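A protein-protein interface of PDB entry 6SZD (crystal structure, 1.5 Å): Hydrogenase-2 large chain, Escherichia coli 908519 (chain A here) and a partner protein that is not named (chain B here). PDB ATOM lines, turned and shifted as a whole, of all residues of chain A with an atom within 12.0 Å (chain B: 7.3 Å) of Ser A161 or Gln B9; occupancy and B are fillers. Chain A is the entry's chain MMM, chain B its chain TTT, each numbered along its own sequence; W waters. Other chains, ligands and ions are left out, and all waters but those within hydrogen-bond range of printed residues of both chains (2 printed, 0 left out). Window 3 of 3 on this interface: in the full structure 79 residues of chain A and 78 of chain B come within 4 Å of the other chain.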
ATOM      1  N   ILE A 119      13.770  20.785  -2.248  1.00  0.00           N
ATOM      2  CA  ILE A 119      14.510  20.707  -0.949  1.00  0.00           C
ATOM      3  C   ILE A 119      13.806  21.561   0.112  1.00  0.00           C
ATOM      4  O   ILE A 119      13.865  21.180   1.281  1.00  0.00           O
ATOM      5  CB  ILE A 119      15.997  21.075  -1.100  1.00  0.00           C
ATOM      6  CG1 ILE A 119      16.185  22.513  -1.583  1.00  0.00           C
ATOM      7  CG2 ILE A 119      16.710  20.060  -1.987  1.00  0.00           C
ATOM      8  CD1 ILE A 119      16.576  23.491  -0.484  1.00  0.00           C
ATOM      9  N   LEU A 123      11.972  20.625   4.412  1.00  0.00           N
ATOM     10  CA  LEU A 123      11.935  21.310   5.738  1.00  0.00           C
ATOM     11  C   LEU A 123      10.600  21.081   6.465  1.00  0.00           C
ATOM     12  O   LEU A 123      10.592  21.130   7.687  1.00  0.00           O
ATOM     13  CB  LEU A 123      12.201  22.804   5.546  1.00  0.00           C
ATOM     14  CG  LEU A 123      13.617  23.150   5.100  1.00  0.00           C
ATOM     15  CD1 LEU A 123      13.747  24.625   4.779  1.00  0.00           C
ATOM     16  CD2 LEU A 123      14.627  22.723   6.158  1.00  0.00           C
ATOM     17  N   GLN A 152      17.764  16.728   7.767  1.00  0.00           N
ATOM     18  CA  GLN A 152      16.829  17.894   7.768  1.00  0.00           C
ATOM     19  C   GLN A 152      17.558  19.072   8.411  1.00  0.00           C
ATOM     20  O   GLN A 152      17.453  20.194   7.908  1.00  0.00           O
ATOM     21  CB  GLN A 152      15.526  17.537   8.481  1.00  0.00           C
ATOM     22  CG  GLN A 152      14.462  18.612   8.336  1.00  0.00           C
ATOM     23  CD  GLN A 152      13.154  18.202   8.964  1.00  0.00           C
ATOM     24  OE1 GLN A 152      13.095  17.885  10.155  1.00  0.00           O
ATOM     25  NE2 GLN A 152      12.103  18.162   8.142  1.00  0.00           N
ATOM     26  N   ASN A 153      18.274  18.826   9.511  1.00  0.00           N
ATOM     27  CA  ASN A 153      19.029  19.894  10.230  1.00  0.00           C
ATOM     28  C   ASN A 153      20.133  20.466   9.345  1.00  0.00           C
ATOM     29  O   ASN A 153      20.364  21.663   9.427  1.00  0.00           O
ATOM     30  CB  ASN A 153      19.526  19.405  11.591  1.00  0.00           C
ATOM     31  CG  ASN A 153      18.403  19.147  12.571  1.00  0.00           C
ATOM     32  OD1 ASN A 153      17.287  19.634  12.381  1.00  0.00           O
ATOM     33  ND2 ASN A 153      18.697  18.388  13.614  1.00  0.00           N
ATOM     34  N   LYS A 154      20.815  19.662   8.520  1.00  0.00           N
ATOM     35  CA  LYS A 154      21.827  20.217   7.595  1.00  0.00           C
ATOM     36  C   LYS A 154      21.128  21.179   6.633  1.00  0.00           C
ATOM     37  O   LYS A 154      21.714  22.209   6.307  1.00  0.00           O
ATOM     38  CB  LYS A 154      22.541  19.122   6.784  1.00  0.00           C
ATOM     39  CG  LYS A 154      23.401  18.162   7.589  1.00  0.00           C
ATOM     40  CD  LYS A 154      23.891  17.000   6.716  1.00  0.00           C
ATOM     41  CE  LYS A 154      24.798  16.036   7.437  1.00  0.00           C
ATOM     42  NZ  LYS A 154      26.094  16.683   7.746  1.00  0.00           N
ATOM     43  N   ILE A 155      19.946  20.825   6.131  1.00  0.00           N
ATOM     44  CA  ILE A 155      19.205  21.706   5.189  1.00  0.00           C
ATOM     45  C   ILE A 155      18.833  22.983   5.951  1.00  0.00           C
ATOM     46  O   ILE A 155      19.049  24.063   5.416  1.00  0.00           O
ATOM     47  CB  ILE A 155      17.933  21.041   4.634  1.00  0.00           C
ATOM     48  CG1 ILE A 155      18.202  19.723   3.916  1.00  0.00           C
ATOM     49  CG2 ILE A 155      17.183  22.018   3.708  1.00  0.00           C
ATOM     50  CD1 ILE A 155      16.934  18.942   3.665  1.00  0.00           C
ATOM     51  N   LYS A 156      18.244  22.836   7.134  1.00  0.00           N
ATOM     52  CA  LYS A 156      17.872  23.980   8.017  1.00  0.00           C
ATOM     53  C   LYS A 156      19.068  24.914   8.173  1.00  0.00           C
ATOM     54  O   LYS A 156      18.909  26.126   7.934  1.00  0.00           O
ATOM     55  CB  LYS A 156      17.395  23.508   9.391  1.00  0.00           C
ATOM     56  CG  LYS A 156      15.964  23.023   9.441  1.00  0.00           C
ATOM     57  CD  LYS A 156      15.527  22.618  10.842  1.00  0.00           C
ATOM     58  CE  LYS A 156      15.151  23.804  11.698  1.00  0.00           C
ATOM     59  NZ  LYS A 156      14.434  23.374  12.928  1.00  0.00           N
ATOM     60  N   ASP A 157      20.238  24.382   8.506  1.00  0.00           N
ATOM     61  CA  ASP A 157      21.462  25.189   8.761  1.00  0.00           C
ATOM     62  C   ASP A 157      21.868  25.916   7.476  1.00  0.00           C
ATOM     63  O   ASP A 157      22.270  27.083   7.552  1.00  0.00           O
ATOM     64  CB  ASP A 157      22.619  24.338   9.300  1.00  0.00           C
ATOM     65  CG  ASP A 157      22.364  23.737  10.680  1.00  0.00           C
ATOM     66  OD1 ASP A 157      21.479  24.236  11.385  1.00  0.00           O
ATOM     67  OD2 ASP A 157      23.054  22.766  11.040  1.00  0.00           O
ATOM     68  N   LEU A 158      21.820  25.239   6.321  1.00  0.00           N
ATOM     69  CA  LEU A 158      22.212  25.888   5.047  1.00  0.00           C
ATOM     70  C   LEU A 158      21.244  27.057   4.789  1.00  0.00           C
ATOM     71  O   LEU A 158      21.753  28.159   4.518  1.00  0.00           O
ATOM     72  CB  LEU A 158      22.212  24.867   3.910  1.00  0.00           C
ATOM     73  CG  LEU A 158      22.740  25.390   2.577  1.00  0.00           C
ATOM     74  CD1 LEU A 158      24.256  25.410   2.582  1.00  0.00           C
ATOM     75  CD2 LEU A 158      22.263  24.536   1.429  1.00  0.00           C
ATOM     76  N   VAL A 159      19.929  26.818   4.858  1.00  0.00           N
ATOM     77  CA  VAL A 159      18.892  27.879   4.625  1.00  0.00           C
ATOM     78  C   VAL A 159      19.125  29.025   5.630  1.00  0.00           C
ATOM     79  O   VAL A 159      19.248  30.190   5.191  1.00  0.00           O
ATOM     80  CB  VAL A 159      17.459  27.305   4.676  1.00  0.00           C
ATOM     81  CG1 VAL A 159      16.391  28.385   4.535  1.00  0.00           C
ATOM     82  CG2 VAL A 159      17.251  26.257   3.598  1.00  0.00           C
ATOM     83  N   ALA A 160      19.334  28.710   6.909  1.00  0.00           N
ATOM     84  CA  ALA A 160      19.571  29.701   7.989  1.00  0.00           C
ATOM     85  C   ALA A 160      20.794  30.581   7.684  1.00  0.00           C
ATOM     86  O   ALA A 160      20.786  31.755   8.094  1.00  0.00           O
ATOM     87  CB  ALA A 160      19.699  29.004   9.325  1.00  0.00           C
ATOM     88  N   SER A 161      21.816  30.066   6.993  1.00  0.00           N
ATOM     89  CA  SER A 161      23.059  30.826   6.700  1.00  0.00           C
ATOM     90  C   SER A 161      22.766  31.924   5.676  1.00  0.00           C
ATOM     91  O   SER A 161      23.599  32.807   5.519  1.00  0.00           O
ATOM     92  CB  SER A 161      24.151  29.920   6.195  1.00  0.00           C
ATOM     93  OG  SER A 161      23.954  29.629   4.803  1.00  0.00           O
ATOM     94  N   GLY A 162      21.666  31.814   4.943  1.00  0.00           N
ATOM     95  CA  GLY A 162      21.359  32.707   3.809  1.00  0.00           C
ATOM     96  C   GLY A 162      22.279  32.500   2.611  1.00  0.00           C
ATOM     97  O   GLY A 162      22.175  33.291   1.670  1.00  0.00           O
ATOM     98  N   GLN A 163      23.168  31.497   2.630  1.00  0.00           N
ATOM     99  CA  GLN A 163      24.059  31.186   1.480  1.00  0.00           C
ATOM    100  C   GLN A 163      23.647  29.844   0.893  1.00  0.00           C
ATOM    101  O   GLN A 163      24.194  28.814   1.333  1.00  0.00           O
ATOM    102  CB  GLN A 163      25.522  31.126   1.904  1.00  0.00           C
ATOM    103  CG  GLN A 163      26.112  32.471   2.305  1.00  0.00           C
ATOM    104  CD  GLN A 163      27.542  32.257   2.714  1.00  0.00           C
ATOM    105  OE1 GLN A 163      27.803  31.594   3.722  1.00  0.00           O
ATOM    106  NE2 GLN A 163      28.454  32.756   1.903  1.00  0.00           N
ATOM    107  N   LEU A 164      22.698  29.845  -0.046  1.00  0.00           N
ATOM    108  CA  LEU A 164      22.150  28.580  -0.615  1.00  0.00           C
ATOM    109  C   LEU A 164      23.106  28.060  -1.714  1.00  0.00           C
ATOM    110  O   LEU A 164      23.056  26.860  -2.003  1.00  0.00           O
ATOM    111  CB  LEU A 164      20.736  28.812  -1.171  1.00  0.00           C
ATOM    112  CG  LEU A 164      19.706  29.389  -0.188  1.00  0.00           C
ATOM    113  CD1 LEU A 164      18.377  29.697  -0.883  1.00  0.00           C
ATOM    114  CD2 LEU A 164      19.497  28.438   0.959  1.00  0.00           C
ATOM    115  N   GLY A 165      23.930  28.941  -2.267  1.00  0.00           N
ATOM    116  CA  GLY A 165      24.914  28.654  -3.329  1.00  0.00           C
ATOM    117  C   GLY A 165      24.261  27.850  -4.452  1.00  0.00           C
ATOM    118  O   GLY A 165      23.234  28.272  -4.975  1.00  0.00           O
ATOM    119  N   ILE A 166      24.760  26.673  -4.727  1.00  0.00           N
ATOM    120  CA  ILE A 166      24.284  25.831  -5.864  1.00  0.00           C
ATOM    121  C   ILE A 166      22.856  25.311  -5.623  1.00  0.00           C
ATOM    122  O   ILE A 166      22.243  24.832  -6.597  1.00  0.00           O
ATOM    123  CB  ILE A 166      25.287  24.686  -6.123  1.00  0.00           C
ATOM    124  CG1 ILE A 166      25.593  23.888  -4.857  1.00  0.00           C
ATOM    125  CG2 ILE A 166      26.553  25.242  -6.761  1.00  0.00           C
ATOM    126  CD1 ILE A 166      26.358  22.623  -5.111  1.00  0.00           C
ATOM    127  N   PHE A 167      22.298  25.424  -4.414  1.00  0.00           N
ATOM    128  CA  PHE A 167      20.873  25.090  -4.176  1.00  0.00           C
ATOM    129  C   PHE A 167      19.984  26.330  -4.363  1.00  0.00           C
ATOM    130  O   PHE A 167      18.750  26.198  -4.264  1.00  0.00           O
ATOM    131  CB  PHE A 167      20.707  24.408  -2.819  1.00  0.00           C
ATOM    132  CG  PHE A 167      21.599  23.209  -2.692  1.00  0.00           C
ATOM    133  CD1 PHE A 167      21.221  22.006  -3.263  1.00  0.00           C
ATOM    134  CD2 PHE A 167      22.860  23.311  -2.125  1.00  0.00           C
ATOM    135  CE1 PHE A 167      22.058  20.901  -3.195  1.00  0.00           C
ATOM    136  CE2 PHE A 167      23.704  22.209  -2.072  1.00  0.00           C
ATOM    137  CZ  PHE A 167      23.303  21.008  -2.616  1.00  0.00           C
ATOM    138  N   ALA A 168      20.537  27.485  -4.700  1.00  0.00           N
ATOM    139  CA  ALA A 168      19.770  28.766  -4.792  1.00  0.00           C
ATOM    140  C   ALA A 168      18.927  28.820  -6.071  1.00  0.00           C
ATOM    141  O   ALA A 168      19.390  28.332  -7.134  1.00  0.00           O
ATOM    142  CB  ALA A 168      20.702  29.949  -4.768  1.00  0.00           C
ATOM    143  N   PRO B   8      27.295  30.816  10.580  1.00  0.00           N
ATOM    144  CA  PRO B   8      28.497  31.571  10.128  1.00  0.00           C
ATOM    145  C   PRO B   8      28.653  31.565   8.592  1.00  0.00           C
ATOM    146  O   PRO B   8      28.286  30.583   7.974  1.00  0.00           O
ATOM    147  CB  PRO B   8      29.692  30.874  10.813  1.00  0.00           C
ATOM    148  CG  PRO B   8      29.190  29.467  11.106  1.00  0.00           C
ATOM    149  CD  PRO B   8      27.692  29.602  11.318  1.00  0.00           C
ATOM    150  N   GLN B   9      29.168  32.653   8.012  1.00  0.00           N
ATOM    151  CA  GLN B   9      29.276  32.813   6.534  1.00  0.00           C
ATOM    152  C   GLN B   9      30.479  32.017   6.003  1.00  0.00           C
ATOM    153  O   GLN B   9      31.543  32.016   6.626  1.00  0.00           O
ATOM    154  CB  GLN B   9      29.340  34.291   6.145  1.00  0.00           C
ATOM    155  CG  GLN B   9      28.097  35.063   6.601  1.00  0.00           C
ATOM    156  CD  GLN B   9      26.807  34.540   6.007  1.00  0.00           C
ATOM    157  OE1 GLN B   9      26.526  34.727   4.823  1.00  0.00           O
ATOM    158  NE2 GLN B   9      26.000  33.882   6.831  1.00  0.00           N
ATOM    159  N   ARG B  10      30.294  31.325   4.887  1.00  0.00           N
ATOM    160  CA  ARG B  10      31.363  30.504   4.275  1.00  0.00           C
ATOM    161  C   ARG B  10      31.969  31.286   3.120  1.00  0.00           C
ATOM    162  O   ARG B  10      31.280  32.031   2.409  1.00  0.00           O
ATOM    163  CB  ARG B  10      30.761  29.176   3.828  1.00  0.00           C
ATOM    164  CG  ARG B  10      30.491  28.213   4.977  1.00  0.00           C
ATOM    165  CD  ARG B  10      29.558  27.083   4.638  1.00  0.00           C
ATOM    166  NE  ARG B  10      28.198  27.579   4.502  1.00  0.00           N
ATOM    167  CZ  ARG B  10      27.443  27.530   3.421  1.00  0.00           C
ATOM    168  NH1 ARG B  10      27.850  26.951   2.307  1.00  0.00           N
ATOM    169  NH2 ARG B  10      26.221  28.020   3.486  1.00  0.00           N
ATOM    170  N   PRO B  11      33.271  31.130   2.862  1.00  0.00           N
ATOM    171  CA  PRO B  11      33.937  31.885   1.804  1.00  0.00           C
ATOM    172  C   PRO B  11      33.370  31.493   0.439  1.00  0.00           C
ATOM    173  O   PRO B  11      33.214  30.312   0.103  1.00  0.00           O
ATOM    174  CB  PRO B  11      35.427  31.533   1.875  1.00  0.00           C
ATOM    175  CG  PRO B  11      35.538  30.482   2.978  1.00  0.00           C
ATOM    176  CD  PRO B  11      34.189  30.285   3.641  1.00  0.00           C
ATOM    177  N   PRO B  12      32.996  32.503  -0.379  1.00  0.00           N
ATOM    178  CA  PRO B  12      32.357  32.211  -1.663  1.00  0.00           C
ATOM    179  C   PRO B  12      33.369  31.769  -2.734  1.00  0.00           C
ATOM    180  O   PRO B  12      34.511  32.253  -2.801  1.00  0.00           O
ATOM    181  CB  PRO B  12      31.698  33.562  -1.979  1.00  0.00           C
ATOM    182  CG  PRO B  12      32.660  34.562  -1.404  1.00  0.00           C
ATOM    183  CD  PRO B  12      33.114  33.948  -0.096  1.00  0.00           C
ATOM    184  N   LEU B  41      28.921  22.193   1.979  1.00  0.00           N
ATOM    185  CA  LEU B  41      28.031  22.517   3.134  1.00  0.00           C
ATOM    186  C   LEU B  41      28.807  23.232   4.243  1.00  0.00           C
ATOM    187  O   LEU B  41      28.171  23.984   4.983  1.00  0.00           O
ATOM    188  CB  LEU B  41      27.380  21.249   3.667  1.00  0.00           C
ATOM    189  CG  LEU B  41      26.424  20.552   2.696  1.00  0.00           C
ATOM    190  CD1 LEU B  41      25.752  19.380   3.359  1.00  0.00           C
ATOM    191  CD2 LEU B  41      25.376  21.506   2.146  1.00  0.00           C
ATOM    192  N   GLU B  42      30.117  22.988   4.385  1.00  0.00           N
ATOM    193  CA  GLU B  42      30.875  23.450   5.581  1.00  0.00           C
ATOM    194  C   GLU B  42      32.022  24.369   5.202  1.00  0.00           C
ATOM    195  O   GLU B  42      32.202  25.367   5.891  1.00  0.00           O
ATOM    196  CB  GLU B  42      31.392  22.283   6.425  1.00  0.00           C
ATOM    197  CG  GLU B  42      30.308  21.308   6.805  1.00  0.00           C
ATOM    198  CD  GLU B  42      30.699  20.115   7.665  1.00  0.00           C
ATOM    199  OE1 GLU B  42      31.909  19.808   7.762  1.00  0.00           O
ATOM    200  OE2 GLU B  42      29.772  19.474   8.209  1.00  0.00           O
ATOM    201  N   THR B  43      32.827  24.046   4.206  1.00  0.00           N
ATOM    202  CA  THR B  43      34.110  24.750   3.958  1.00  0.00           C
ATOM    203  C   THR B  43      33.884  26.039   3.154  1.00  0.00           C
ATOM    204  O   THR B  43      34.471  27.088   3.499  1.00  0.00           O
ATOM    205  CB  THR B  43      35.106  23.842   3.242  1.00  0.00           C
ATOM    206  OG1 THR B  43      35.089  22.578   3.918  1.00  0.00           O
ATOM    207  CG2 THR B  43      36.476  24.475   3.204  1.00  0.00           C
ATOM    208  N   ILE B  44      33.123  25.947   2.066  1.00  0.00           N
ATOM    209  CA  ILE B  44      32.944  27.091   1.125  1.00  0.00           C
ATOM    210  C   ILE B  44      31.446  27.301   0.915  1.00  0.00           C
ATOM    211  O   ILE B  44      30.623  26.457   1.253  1.00  0.00           O
ATOM    212  CB  ILE B  44      33.683  26.878  -0.213  1.00  0.00           C
ATOM    213  CG1 ILE B  44      33.086  25.705  -1.007  1.00  0.00           C
ATOM    214  CG2 ILE B  44      35.178  26.768  -0.004  1.00  0.00           C
ATOM    215  CD1 ILE B  44      33.599  25.523  -2.421  1.00  0.00           C
ATOM    216  N   SER B  45      31.119  28.405   0.262  1.00  0.00           N
ATOM    217  CA  SER B  45      29.818  28.575  -0.418  1.00  0.00           C
ATOM    218  C   SER B  45      30.097  28.532  -1.916  1.00  0.00           C
ATOM    219  O   SER B  45      30.746  29.461  -2.444  1.00  0.00           O
ATOM    220  CB  SER B  45      29.121  29.865  -0.016  1.00  0.00           C
ATOM    221  OG  SER B  45      27.871  29.950  -0.667  1.00  0.00           O
ATOM    222  N   LYS B  70      27.455  40.808  -5.011  1.00  0.00           N
ATOM    223  CA  LYS B  70      27.416  40.617  -3.541  1.00  0.00           C
ATOM    224  C   LYS B  70      28.825  40.358  -2.984  1.00  0.00           C
ATOM    225  O   LYS B  70      29.139  40.888  -1.912  1.00  0.00           O
ATOM    226  CB  LYS B  70      26.490  39.458  -3.196  1.00  0.00           C
ATOM    227  CG  LYS B  70      26.283  39.250  -1.704  1.00  0.00           C
ATOM    228  CD  LYS B  70      25.232  38.231  -1.374  1.00  0.00           C
ATOM    229  CE  LYS B  70      25.176  37.948   0.106  1.00  0.00           C
ATOM    230  NZ  LYS B  70      24.351  36.755   0.398  1.00  0.00           N
ATOM    231  N   TYR B  71      29.640  39.520  -3.637  1.00  0.00           N
ATOM    232  CA  TYR B  71      30.917  39.029  -3.054  1.00  0.00           C
ATOM    233  C   TYR B  71      32.110  39.690  -3.750  1.00  0.00           C
ATOM    234  O   TYR B  71      33.255  39.203  -3.685  1.00  0.00           O
ATOM    235  CB  TYR B  71      30.960  37.500  -3.119  1.00  0.00           C
ATOM    236  CG  TYR B  71      29.899  36.807  -2.315  1.00  0.00           C
ATOM    237  CD1 TYR B  71      29.908  36.875  -0.928  1.00  0.00           C
ATOM    238  CD2 TYR B  71      28.911  36.046  -2.922  1.00  0.00           C
ATOM    239  CE1 TYR B  71      28.951  36.219  -0.165  1.00  0.00           C
ATOM    240  CE2 TYR B  71      27.966  35.370  -2.174  1.00  0.00           C
ATOM    241  CZ  TYR B  71      27.978  35.463  -0.787  1.00  0.00           C
ATOM    242  OH  TYR B  71      27.043  34.800  -0.038  1.00  0.00           O
HETATM  243  O   HOH W   1      27.118  29.884   5.687  1.00  0.00           O
HETATM  244  O   HOH W   2      26.163  27.610  -0.037  1.00  0.00           O
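CD1 of Leu A158 touches NH2 of Arg B10, at 3.4 Å.
Gln A163 touches Gln B9 (OE1 to CA, 3.4 Å).
Gln A163 touches Ser B45 (NE2 to CB, 3.5 Å).
The side-chain amide oxygen (OE1) of Gln A163 is in hydrogen-bond range of the backbone NH (N) of Arg B10 (2.8 Å).
The side-chain hydroxyl (OH) of Tyr B71 lies within hydrogen-bond range of the side-chain amide nitrogen (NE2) of Gln A163 (3.2 Å).
NE2 of Gln B9 lies within hydrogen-bond range of O of Ser A161 (2.9 Å).
The guanidinium group (NH2) of Arg B10 sits at hydrogen-bond distance from the side-chain hydroxyl (OG) of Ser A161 (3.1 Å).
Ser A161 touches just these residues of chain B: Gln B9 and Arg B10.
Of chain A, only Ser A161 and Gln A163 come within 4 Å of Gln B9.
No residue of chain A comes within 4 Å of Pro B8.
Of the printed residues of chain B, Gln A163 touches Gln B9 (3.4 Å), Arg B10 (2.8 Å), Ser B45 (3.5 Å) and Tyr B71 (3.2 Å).
Printed residues of chain A within 4 Å of Ser B45: Gln A163.
Ile B44 touches none of the printed residues of chain A.
Leu B41 touches none of the printed residues of chain A.
The nearest residue of chain B that does not touch Ser A161 is Pro B8 (4.6 Å).
The nearest residue of chain A that does not touch Gln B9 is Gly A162 (5.2 Å).
Hydrophobic or aromatic side chains of chain A within 4 Å of the printed part of chain B: Leu A158.
Among the printed residues, 7 pairs touch across the chains.
Among the printed residues, no Asp or Glu carboxylate lies within 4 Å of a Lys or Arg side-chain nitrogen of the other chain.
The side-chain hydroxyl (OG) of Ser A161 lies within hydrogen-bond range of the backbone carbonyl oxygen (O) of Leu A158 (2.7 Å).
The backbone carbonyl oxygen (O) of Pro B11 sits at hydrogen-bond distance from the backbone NH (N) of Ser B45 (2.8 Å).
OG of Ser A161 is in hydrogen-bond range of N of Gln A163.
The guanidinium group (NH1) of Arg B10 sits at hydrogen-bond distance from the backbone carbonyl oxygen (O) of Ile B44, 3.0 Å away.
OH of Tyr B71 lies within hydrogen-bond range of NZ of Lys B70 (3.4 Å).
Water W1 lies within hydrogen-bond range of the backbone carbonyl oxygen (O) of Pro B8, the side-chain amide oxygen (OE1) of Gln A163, the guanidinium group (NE) of Arg B10 and the side-chain hydroxyl (OG) of Ser A161.
Water W2 lies within hydrogen-bond range of O of Gln A163, NH1 of Arg B10, OG of Ser B45 and N of Gly A165.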
